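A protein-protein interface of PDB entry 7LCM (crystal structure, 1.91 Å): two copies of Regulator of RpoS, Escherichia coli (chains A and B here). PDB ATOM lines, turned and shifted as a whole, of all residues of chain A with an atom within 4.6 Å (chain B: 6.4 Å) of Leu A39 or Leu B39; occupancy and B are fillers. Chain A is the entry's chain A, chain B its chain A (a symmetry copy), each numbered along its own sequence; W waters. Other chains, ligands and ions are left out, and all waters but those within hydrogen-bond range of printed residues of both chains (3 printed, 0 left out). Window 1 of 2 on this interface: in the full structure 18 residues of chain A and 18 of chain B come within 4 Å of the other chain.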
ATOM      1  N   ILE A  15      -0.135 -10.607   2.711  1.00  0.00           N
ATOM      2  CA  ILE A  15       1.011 -10.042   1.989  1.00  0.00           C
ATOM      3  C   ILE A  15       0.533  -8.804   1.228  1.00  0.00           C
ATOM      4  O   ILE A  15      -0.408  -8.889   0.432  1.00  0.00           O
ATOM      5  CB  ILE A  15       1.629 -11.078   1.027  1.00  0.00           C
ATOM      6  CG1 ILE A  15       2.261 -12.242   1.802  1.00  0.00           C
ATOM      7  CG2 ILE A  15       2.627 -10.430   0.059  1.00  0.00           C
ATOM      8  CD1 ILE A  15       2.154 -13.597   1.091  1.00  0.00           C
ATOM      9  N   ARG A  23       5.096 -10.436  -5.099  1.00  0.00           N
ATOM     10  CA  ARG A  23       3.863 -11.000  -4.561  1.00  0.00           C
ATOM     11  C   ARG A  23       3.810 -12.515  -4.788  1.00  0.00           C
ATOM     12  O   ARG A  23       3.491 -13.293  -3.875  1.00  0.00           O
ATOM     13  CB  ARG A  23       2.688 -10.289  -5.241  1.00  0.00           C
ATOM     14  CG  ARG A  23       1.432 -10.180  -4.454  1.00  0.00           C
ATOM     15  CD  ARG A  23       0.666  -8.929  -4.826  1.00  0.00           C
ATOM     16  NE  ARG A  23       0.221  -8.968  -6.212  1.00  0.00           N
ATOM     17  CZ  ARG A  23       0.424  -7.985  -7.068  1.00  0.00           C
ATOM     18  NH1 ARG A  23       1.092  -6.900  -6.718  1.00  0.00           N
ATOM     19  NH2 ARG A  23      -0.078  -8.077  -8.299  1.00  0.00           N
ATOM     20  N   ASP A  27       4.023 -15.532  -1.888  1.00  0.00           N
ATOM     21  CA  ASP A  27       2.946 -16.517  -1.877  1.00  0.00           C
ATOM     22  C   ASP A  27       3.511 -17.929  -1.953  1.00  0.00           C
ATOM     23  O   ASP A  27       3.175 -18.797  -1.132  1.00  0.00           O
ATOM     24  CB  ASP A  27       1.995 -16.228  -3.042  1.00  0.00           C
ATOM     25  CG  ASP A  27       0.693 -16.999  -2.957  1.00  0.00           C
ATOM     26  OD1 ASP A  27       0.418 -17.648  -1.926  1.00  0.00           O
ATOM     27  OD2 ASP A  27      -0.082 -16.927  -3.930  1.00  0.00           O
ATOM     28  N   THR A  37      -2.502 -17.865   2.507  1.00  0.00           N
ATOM     29  CA  THR A  37      -2.067 -16.514   2.180  1.00  0.00           C
ATOM     30  C   THR A  37      -3.238 -15.722   1.634  1.00  0.00           C
ATOM     31  O   THR A  37      -4.081 -16.260   0.914  1.00  0.00           O
ATOM     32  CB  THR A  37      -0.964 -16.515   1.116  1.00  0.00           C
ATOM     33  OG1 THR A  37      -1.415 -17.265  -0.024  1.00  0.00           O
ATOM     34  CG2 THR A  37       0.319 -17.122   1.645  1.00  0.00           C
ATOM     35  N   VAL A  38      -3.266 -14.436   1.959  1.00  0.00           N
ATOM     36  CA  VAL A  38      -4.121 -13.454   1.309  1.00  0.00           C
ATOM     37  C   VAL A  38      -3.182 -12.391   0.766  1.00  0.00           C
ATOM     38  O   VAL A  38      -2.301 -11.933   1.494  1.00  0.00           O
ATOM     39  CB  VAL A  38      -5.137 -12.851   2.296  1.00  0.00           C
ATOM     40  CG1 VAL A  38      -5.892 -11.704   1.631  1.00  0.00           C
ATOM     41  CG2 VAL A  38      -6.111 -13.933   2.777  1.00  0.00           C
ATOM     42  N   LEU A  39      -3.312 -12.055  -0.519  1.00  0.00           N
ATOM     43  CA  LEU A  39      -2.421 -11.101  -1.155  1.00  0.00           C
ATOM     44  C   LEU A  39      -3.198  -9.887  -1.631  1.00  0.00           C
ATOM     45  O   LEU A  39      -4.247 -10.018  -2.252  1.00  0.00           O
ATOM     46  CB  LEU A  39      -1.693 -11.736  -2.328  1.00  0.00           C
ATOM     47  CG  LEU A  39      -0.767 -12.792  -1.724  1.00  0.00           C
ATOM     48  CD1 LEU A  39      -1.349 -14.188  -1.910  1.00  0.00           C
ATOM     49  CD2 LEU A  39       0.617 -12.668  -2.319  1.00  0.00           C
ATOM     50  N   ALA A  40      -2.649  -8.704  -1.376  1.00  0.00           N
ATOM     51  CA  ALA A  40      -3.243  -7.466  -1.841  1.00  0.00           C
ATOM     52  C   ALA A  40      -2.154  -6.711  -2.581  1.00  0.00           C
ATOM     53  O   ALA A  40      -1.040  -6.561  -2.071  1.00  0.00           O
ATOM     54  CB  ALA A  40      -3.807  -6.646  -0.671  1.00  0.00           C
ATOM     55  N   ALA A  41      -2.448  -6.312  -3.807  1.00  0.00           N
ATOM     56  CA  ALA A  41      -1.490  -5.533  -4.573  1.00  0.00           C
ATOM     57  C   ALA A  41      -1.392  -4.093  -4.089  1.00  0.00           C
ATOM     58  O   ALA A  41      -0.417  -3.409  -4.410  1.00  0.00           O
ATOM     59  CB  ALA A  41      -1.875  -5.578  -6.056  1.00  0.00           C
ATOM     60  N   ILE B  13     -10.397  -7.082  -8.493  1.00  0.00           N
ATOM     61  CA  ILE B  13     -10.720  -8.476  -8.791  1.00  0.00           C
ATOM     62  C   ILE B  13     -10.280  -9.352  -7.630  1.00  0.00           C
ATOM     63  O   ILE B  13      -9.097  -9.344  -7.264  1.00  0.00           O
ATOM     64  CB  ILE B  13     -10.025  -8.975 -10.074  1.00  0.00           C
ATOM     65  CG1 ILE B  13     -10.224  -8.025 -11.265  1.00  0.00           C
ATOM     66  CG2 ILE B  13     -10.478 -10.417 -10.380  1.00  0.00           C
ATOM     67  CD1 ILE B  13     -11.635  -7.745 -11.593  1.00  0.00           C
ATOM     68  N   LEU B  14     -11.197 -10.170  -7.106  1.00  0.00           N
ATOM     69  CA  LEU B  14     -10.848 -11.194  -6.119  1.00  0.00           C
ATOM     70  C   LEU B  14     -10.643 -12.520  -6.838  1.00  0.00           C
ATOM     71  O   LEU B  14     -11.516 -12.946  -7.597  1.00  0.00           O
ATOM     72  CB  LEU B  14     -11.947 -11.347  -5.065  1.00  0.00           C
ATOM     73  CG  LEU B  14     -11.878 -12.575  -4.152  1.00  0.00           C
ATOM     74  CD1 LEU B  14     -10.613 -12.531  -3.297  1.00  0.00           C
ATOM     75  CD2 LEU B  14     -13.141 -12.537  -3.279  1.00  0.00           C
ATOM     76  N   ILE B  15      -9.491 -13.154  -6.614  1.00  0.00           N
ATOM     77  CA  ILE B  15      -9.146 -14.461  -7.185  1.00  0.00           C
ATOM     78  C   ILE B  15      -9.102 -15.483  -6.049  1.00  0.00           C
ATOM     79  O   ILE B  15      -8.369 -15.294  -5.072  1.00  0.00           O
ATOM     80  CB  ILE B  15      -7.796 -14.402  -7.931  1.00  0.00           C
ATOM     81  CG1 ILE B  15      -7.890 -13.508  -9.173  1.00  0.00           C
ATOM     82  CG2 ILE B  15      -7.279 -15.805  -8.277  1.00  0.00           C
ATOM     83  CD1 ILE B  15      -6.599 -12.742  -9.489  1.00  0.00           C
ATOM     84  N   VAL B  16      -9.867 -16.569  -6.164  1.00  0.00           N
ATOM     85  CA  VAL B  16      -9.887 -17.609  -5.123  1.00  0.00           C
ATOM     86  C   VAL B  16      -9.463 -18.924  -5.782  1.00  0.00           C
ATOM     87  O   VAL B  16     -10.173 -19.437  -6.645  1.00  0.00           O
ATOM     88  CB  VAL B  16     -11.271 -17.747  -4.463  1.00  0.00           C
ATOM     89  CG1 VAL B  16     -11.200 -18.671  -3.254  1.00  0.00           C
ATOM     90  CG2 VAL B  16     -11.828 -16.378  -4.044  1.00  0.00           C
ATOM     91  N   PHE B  22      -1.329 -21.286 -10.368  1.00  0.00           N
ATOM     92  CA  PHE B  22      -2.405 -20.642 -11.117  1.00  0.00           C
ATOM     93  C   PHE B  22      -2.796 -19.315 -10.481  1.00  0.00           C
ATOM     94  O   PHE B  22      -3.102 -18.344 -11.184  1.00  0.00           O
ATOM     95  CB  PHE B  22      -3.598 -21.585 -11.218  1.00  0.00           C
ATOM     96  CG  PHE B  22      -4.527 -21.228 -12.321  1.00  0.00           C
ATOM     97  CD1 PHE B  22      -4.065 -21.183 -13.617  1.00  0.00           C
ATOM     98  CD2 PHE B  22      -5.854 -20.922 -12.071  1.00  0.00           C
ATOM     99  CE1 PHE B  22      -4.915 -20.842 -14.643  1.00  0.00           C
ATOM    100  CE2 PHE B  22      -6.692 -20.571 -13.097  1.00  0.00           C
ATOM    101  CZ  PHE B  22      -6.223 -20.533 -14.379  1.00  0.00           C
ATOM    102  N   ARG B  23      -2.801 -19.254  -9.146  1.00  0.00           N
ATOM    103  CA  ARG B  23      -2.987 -17.984  -8.452  1.00  0.00           C
ATOM    104  C   ARG B  23      -2.037 -16.916  -9.005  1.00  0.00           C
ATOM    105  O   ARG B  23      -2.441 -15.777  -9.289  1.00  0.00           O
ATOM    106  CB  ARG B  23      -2.751 -18.228  -6.958  1.00  0.00           C
ATOM    107  CG  ARG B  23      -3.488 -17.347  -6.016  1.00  0.00           C
ATOM    108  CD  ARG B  23      -3.787 -18.068  -4.720  1.00  0.00           C
ATOM    109  NE  ARG B  23      -2.565 -18.414  -4.007  1.00  0.00           N
ATOM    110  CZ  ARG B  23      -2.312 -19.625  -3.548  1.00  0.00           C
ATOM    111  NH1 ARG B  23      -3.155 -20.622  -3.746  1.00  0.00           N
ATOM    112  NH2 ARG B  23      -1.199 -19.837  -2.847  1.00  0.00           N
ATOM    113  N   SER B  24      -0.771 -17.285  -9.209  1.00  0.00           N
ATOM    114  CA  SER B  24       0.206 -16.337  -9.736  1.00  0.00           C
ATOM    115  C   SER B  24      -0.111 -15.956 -11.179  1.00  0.00           C
ATOM    116  O   SER B  24       0.000 -14.783 -11.558  1.00  0.00           O
ATOM    117  CB  SER B  24       1.611 -16.929  -9.633  1.00  0.00           C
ATOM    118  OG  SER B  24       2.590 -16.025 -10.149  1.00  0.00           O
ATOM    119  N   LEU B  26      -3.062 -15.867 -12.767  1.00  0.00           N
ATOM    120  CA  LEU B  26      -4.195 -14.941 -12.818  1.00  0.00           C
ATOM    121  C   LEU B  26      -3.802 -13.558 -12.312  1.00  0.00           C
ATOM    122  O   LEU B  26      -4.173 -12.541 -12.910  1.00  0.00           O
ATOM    123  CB  LEU B  26      -5.383 -15.486 -12.028  1.00  0.00           C
ATOM    124  CG  LEU B  26      -6.013 -16.783 -12.551  1.00  0.00           C
ATOM    125  CD1 LEU B  26      -6.912 -17.372 -11.498  1.00  0.00           C
ATOM    126  CD2 LEU B  26      -6.765 -16.553 -13.860  1.00  0.00           C
ATOM    127  N   ASP B  27      -3.052 -13.500 -11.208  1.00  0.00           N
ATOM    128  CA  ASP B  27      -2.571 -12.217 -10.702  1.00  0.00           C
ATOM    129  C   ASP B  27      -1.803 -11.468 -11.782  1.00  0.00           C
ATOM    130  O   ASP B  27      -2.084 -10.295 -12.068  1.00  0.00           O
ATOM    131  CB  ASP B  27      -1.705 -12.466  -9.464  1.00  0.00           C
ATOM    132  CG  ASP B  27      -1.395 -11.201  -8.688  1.00  0.00           C
ATOM    133  OD1 ASP B  27      -1.966 -10.131  -8.985  1.00  0.00           O
ATOM    134  OD2 ASP B  27      -0.587 -11.289  -7.744  1.00  0.00           O
ATOM    135  N   THR B  37      -5.704  -6.602  -7.641  1.00  0.00           N
ATOM    136  CA  THR B  37      -6.092  -7.976  -7.355  1.00  0.00           C
ATOM    137  C   THR B  37      -6.012  -8.226  -5.863  1.00  0.00           C
ATOM    138  O   THR B  37      -5.120  -7.712  -5.185  1.00  0.00           O
ATOM    139  CB  THR B  37      -5.169  -8.983  -8.049  1.00  0.00           C
ATOM    140  OG1 THR B  37      -3.807  -8.685  -7.700  1.00  0.00           O
ATOM    141  CG2 THR B  37      -5.326  -8.936  -9.555  1.00  0.00           C
ATOM    142  N   VAL B  38      -6.934  -9.039  -5.363  1.00  0.00           N
ATOM    143  CA  VAL B  38      -6.858  -9.632  -4.038  1.00  0.00           C
ATOM    144  C   VAL B  38      -6.916 -11.134  -4.259  1.00  0.00           C
ATOM    145  O   VAL B  38      -7.776 -11.604  -5.005  1.00  0.00           O
ATOM    146  CB  VAL B  38      -8.014  -9.155  -3.140  1.00  0.00           C
ATOM    147  CG1 VAL B  38      -8.008  -9.931  -1.826  1.00  0.00           C
ATOM    148  CG2 VAL B  38      -7.895  -7.650  -2.880  1.00  0.00           C
ATOM    149  N   LEU B  39      -5.969 -11.878  -3.683  1.00  0.00           N
ATOM    150  CA  LEU B  39      -5.892 -13.314  -3.887  1.00  0.00           C
ATOM    151  C   LEU B  39      -6.082 -14.045  -2.572  1.00  0.00           C
ATOM    152  O   LEU B  39      -5.478 -13.693  -1.564  1.00  0.00           O
ATOM    153  CB  LEU B  39      -4.558 -13.704  -4.503  1.00  0.00           C
ATOM    154  CG  LEU B  39      -4.557 -13.107  -5.911  1.00  0.00           C
ATOM    155  CD1 LEU B  39      -3.701 -11.849  -5.963  1.00  0.00           C
ATOM    156  CD2 LEU B  39      -4.102 -14.146  -6.911  1.00  0.00           C
ATOM    157  N   ALA B  40      -6.892 -15.099  -2.600  1.00  0.00           N
ATOM    158  CA  ALA B  40      -7.105 -15.937  -1.436  1.00  0.00           C
ATOM    159  C   ALA B  40      -6.838 -17.365  -1.871  1.00  0.00           C
ATOM    160  O   ALA B  40      -7.355 -17.812  -2.899  1.00  0.00           O
ATOM    161  CB  ALA B  40      -8.527 -15.768  -0.882  1.00  0.00           C
ATOM    162  N   ALA B  41      -5.973 -18.048  -1.141  1.00  0.00           N
ATOM    163  CA  ALA B  41      -5.696 -19.441  -1.446  1.00  0.00           C
ATOM    164  C   ALA B  41      -6.832 -20.365  -1.029  1.00  0.00           C
ATOM    165  O   ALA B  41      -6.894 -21.504  -1.501  1.00  0.00           O
ATOM    166  CB  ALA B  41      -4.387 -19.856  -0.765  1.00  0.00           C
ATOM    167  N   LEU B  49     -13.277 -12.706   4.070  1.00  0.00           N
ATOM    168  CA  LEU B  49     -12.870 -11.444   3.437  1.00  0.00           C
ATOM    169  C   LEU B  49     -14.059 -10.703   2.839  1.00  0.00           C
ATOM    170  O   LEU B  49     -14.191  -9.480   3.007  1.00  0.00           O
ATOM    171  CB  LEU B  49     -11.848 -11.719   2.339  1.00  0.00           C
ATOM    172  CG  LEU B  49     -10.435 -12.107   2.729  1.00  0.00           C
ATOM    173  CD1 LEU B  49      -9.666 -12.381   1.459  1.00  0.00           C
ATOM    174  CD2 LEU B  49      -9.771 -11.008   3.587  1.00  0.00           C
HETATM  175  O   HOH W   1       0.687 -15.988  -6.343  1.00  0.00           O
HETATM  176  O   HOH W   2      -5.130  -5.124  -3.793  1.00  0.00           O
HETATM  177  O   HOH W   3      -6.576 -17.601   1.695  1.00  0.00           O
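Water W1 bridges OD2 of Asp A27 and N of Ser B24.
Water W2 lies within hydrogen-bond range of the backbone NH (N) of Ala A41 (2.9 Å) and the backbone carbonyl oxygen (O) of Thr B37 (2.9 Å).
Water W3 lies within hydrogen-bond range of N of Ala B41 and O of Thr A37.
The guanidinium group of Arg A23 is in salt-bridge range of the side-chain carboxylate of Asp B27 (2.9 Å).
OD1 of Asp A27 lies within salt-bridge range of NH2 of Arg B23 (2.9 Å).
O of Thr A37 sits at hydrogen-bond distance from N of Ala B41, 3.3 Å away.
N of Ala A41 lies within hydrogen-bond range of O of Thr B37 (3.3 Å).
N of Leu A39 is in hydrogen-bond range of O of Leu B39 (2.9 Å).
Arg A23 touches Thr B37, and with the chains exchanged Thr A37 touches Arg B23.
Thr A37 touches Ala B40, and with the chains exchanged Ala A40 touches Thr B37.
Thr A37 touches Ala B41, and with the chains exchanged Ala A41 touches Thr B37.
Val A38 touches Leu B39, and with the chains exchanged Leu A39 touches Val B38.
Positions printed for both chains: 15, 23, 27, 37, 38, 39, 40 and 41.
Of the 14 pairs that touch across the chains among the printed residues, 13 have their exchanged pair printed and touching as well.
N of Ala A40 sits at hydrogen-bond distance from O of Ile A15, 2.9 Å away.
O of Ile B13 is in hydrogen-bond range of N of Val B38 (2.9 Å).
The side-chain carboxylate (OD1) of Asp B27 lies within hydrogen-bond range of the side-chain hydroxyl (OG1) of Thr B37, 2.7 Å away.
OD1 of Asp A27 lies within hydrogen-bond range of OG1 of Thr A37, at 2.7 Å.
The backbone NH (N) of Ile B15 sits at hydrogen-bond distance from the backbone carbonyl oxygen (O) of Val B38, at 2.8 Å.
N of Ala B40 sits at hydrogen-bond distance from O of Ile B15 (2.9 Å).
Leu B39 touches just these residues of chain A: Thr A37, Val A38 and Leu A39.
Of the printed residues of chain A, Ala B41 touches Thr A37 (3.3 Å).
Of the printed residues of chain A, Arg B23 touches Asp A27 (2.9 Å) and Thr A37 (3.8 Å).
Of the printed residues of chain A, Thr B37 touches Arg A23 (3.8 Å), Leu A39 (3.8 Å), Ala A40 (3.8 Å) and Ala A41 (3.3 Å).
Arg A23 touches Thr B37.
NH2 of Arg B23 touches OG1 of Thr A37, at 3.8 Å.
Thr A37 touches Leu B39 (O to O, 3.8 Å).
Thr A37 touches Ala B40 (O to CA, 3.8 Å).
Val A38 touches Leu B39 (CA to O, 3.2 Å).
Leu B49 touches Val A38.
Leu A39 touches Thr B37 (O to O, 3.8 Å).
CA of Val B38 touches O of Leu A39, 3.2 Å away.
Ala A40 touches Thr B37.
Of the 15 printed residues of chain B, 8 touch a printed residue of chain A.
Of the 8 printed residues of chain A, 7 touch a printed residue of chain B.
Printed residues of chain A that touch a printed residue of chain B: Arg A23, Asp A27, Thr A37, Val A38, Leu A39, Ala A40 and Ala A41.
Among the printed residues, 14 pairs touch across the chains.
Among the printed residues, Asp or Glu carboxylates within 4 Å of a Lys or Arg side-chain nitrogen of the other chain: Arg A23 with Asp B27 and Asp A27 with Arg B23.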
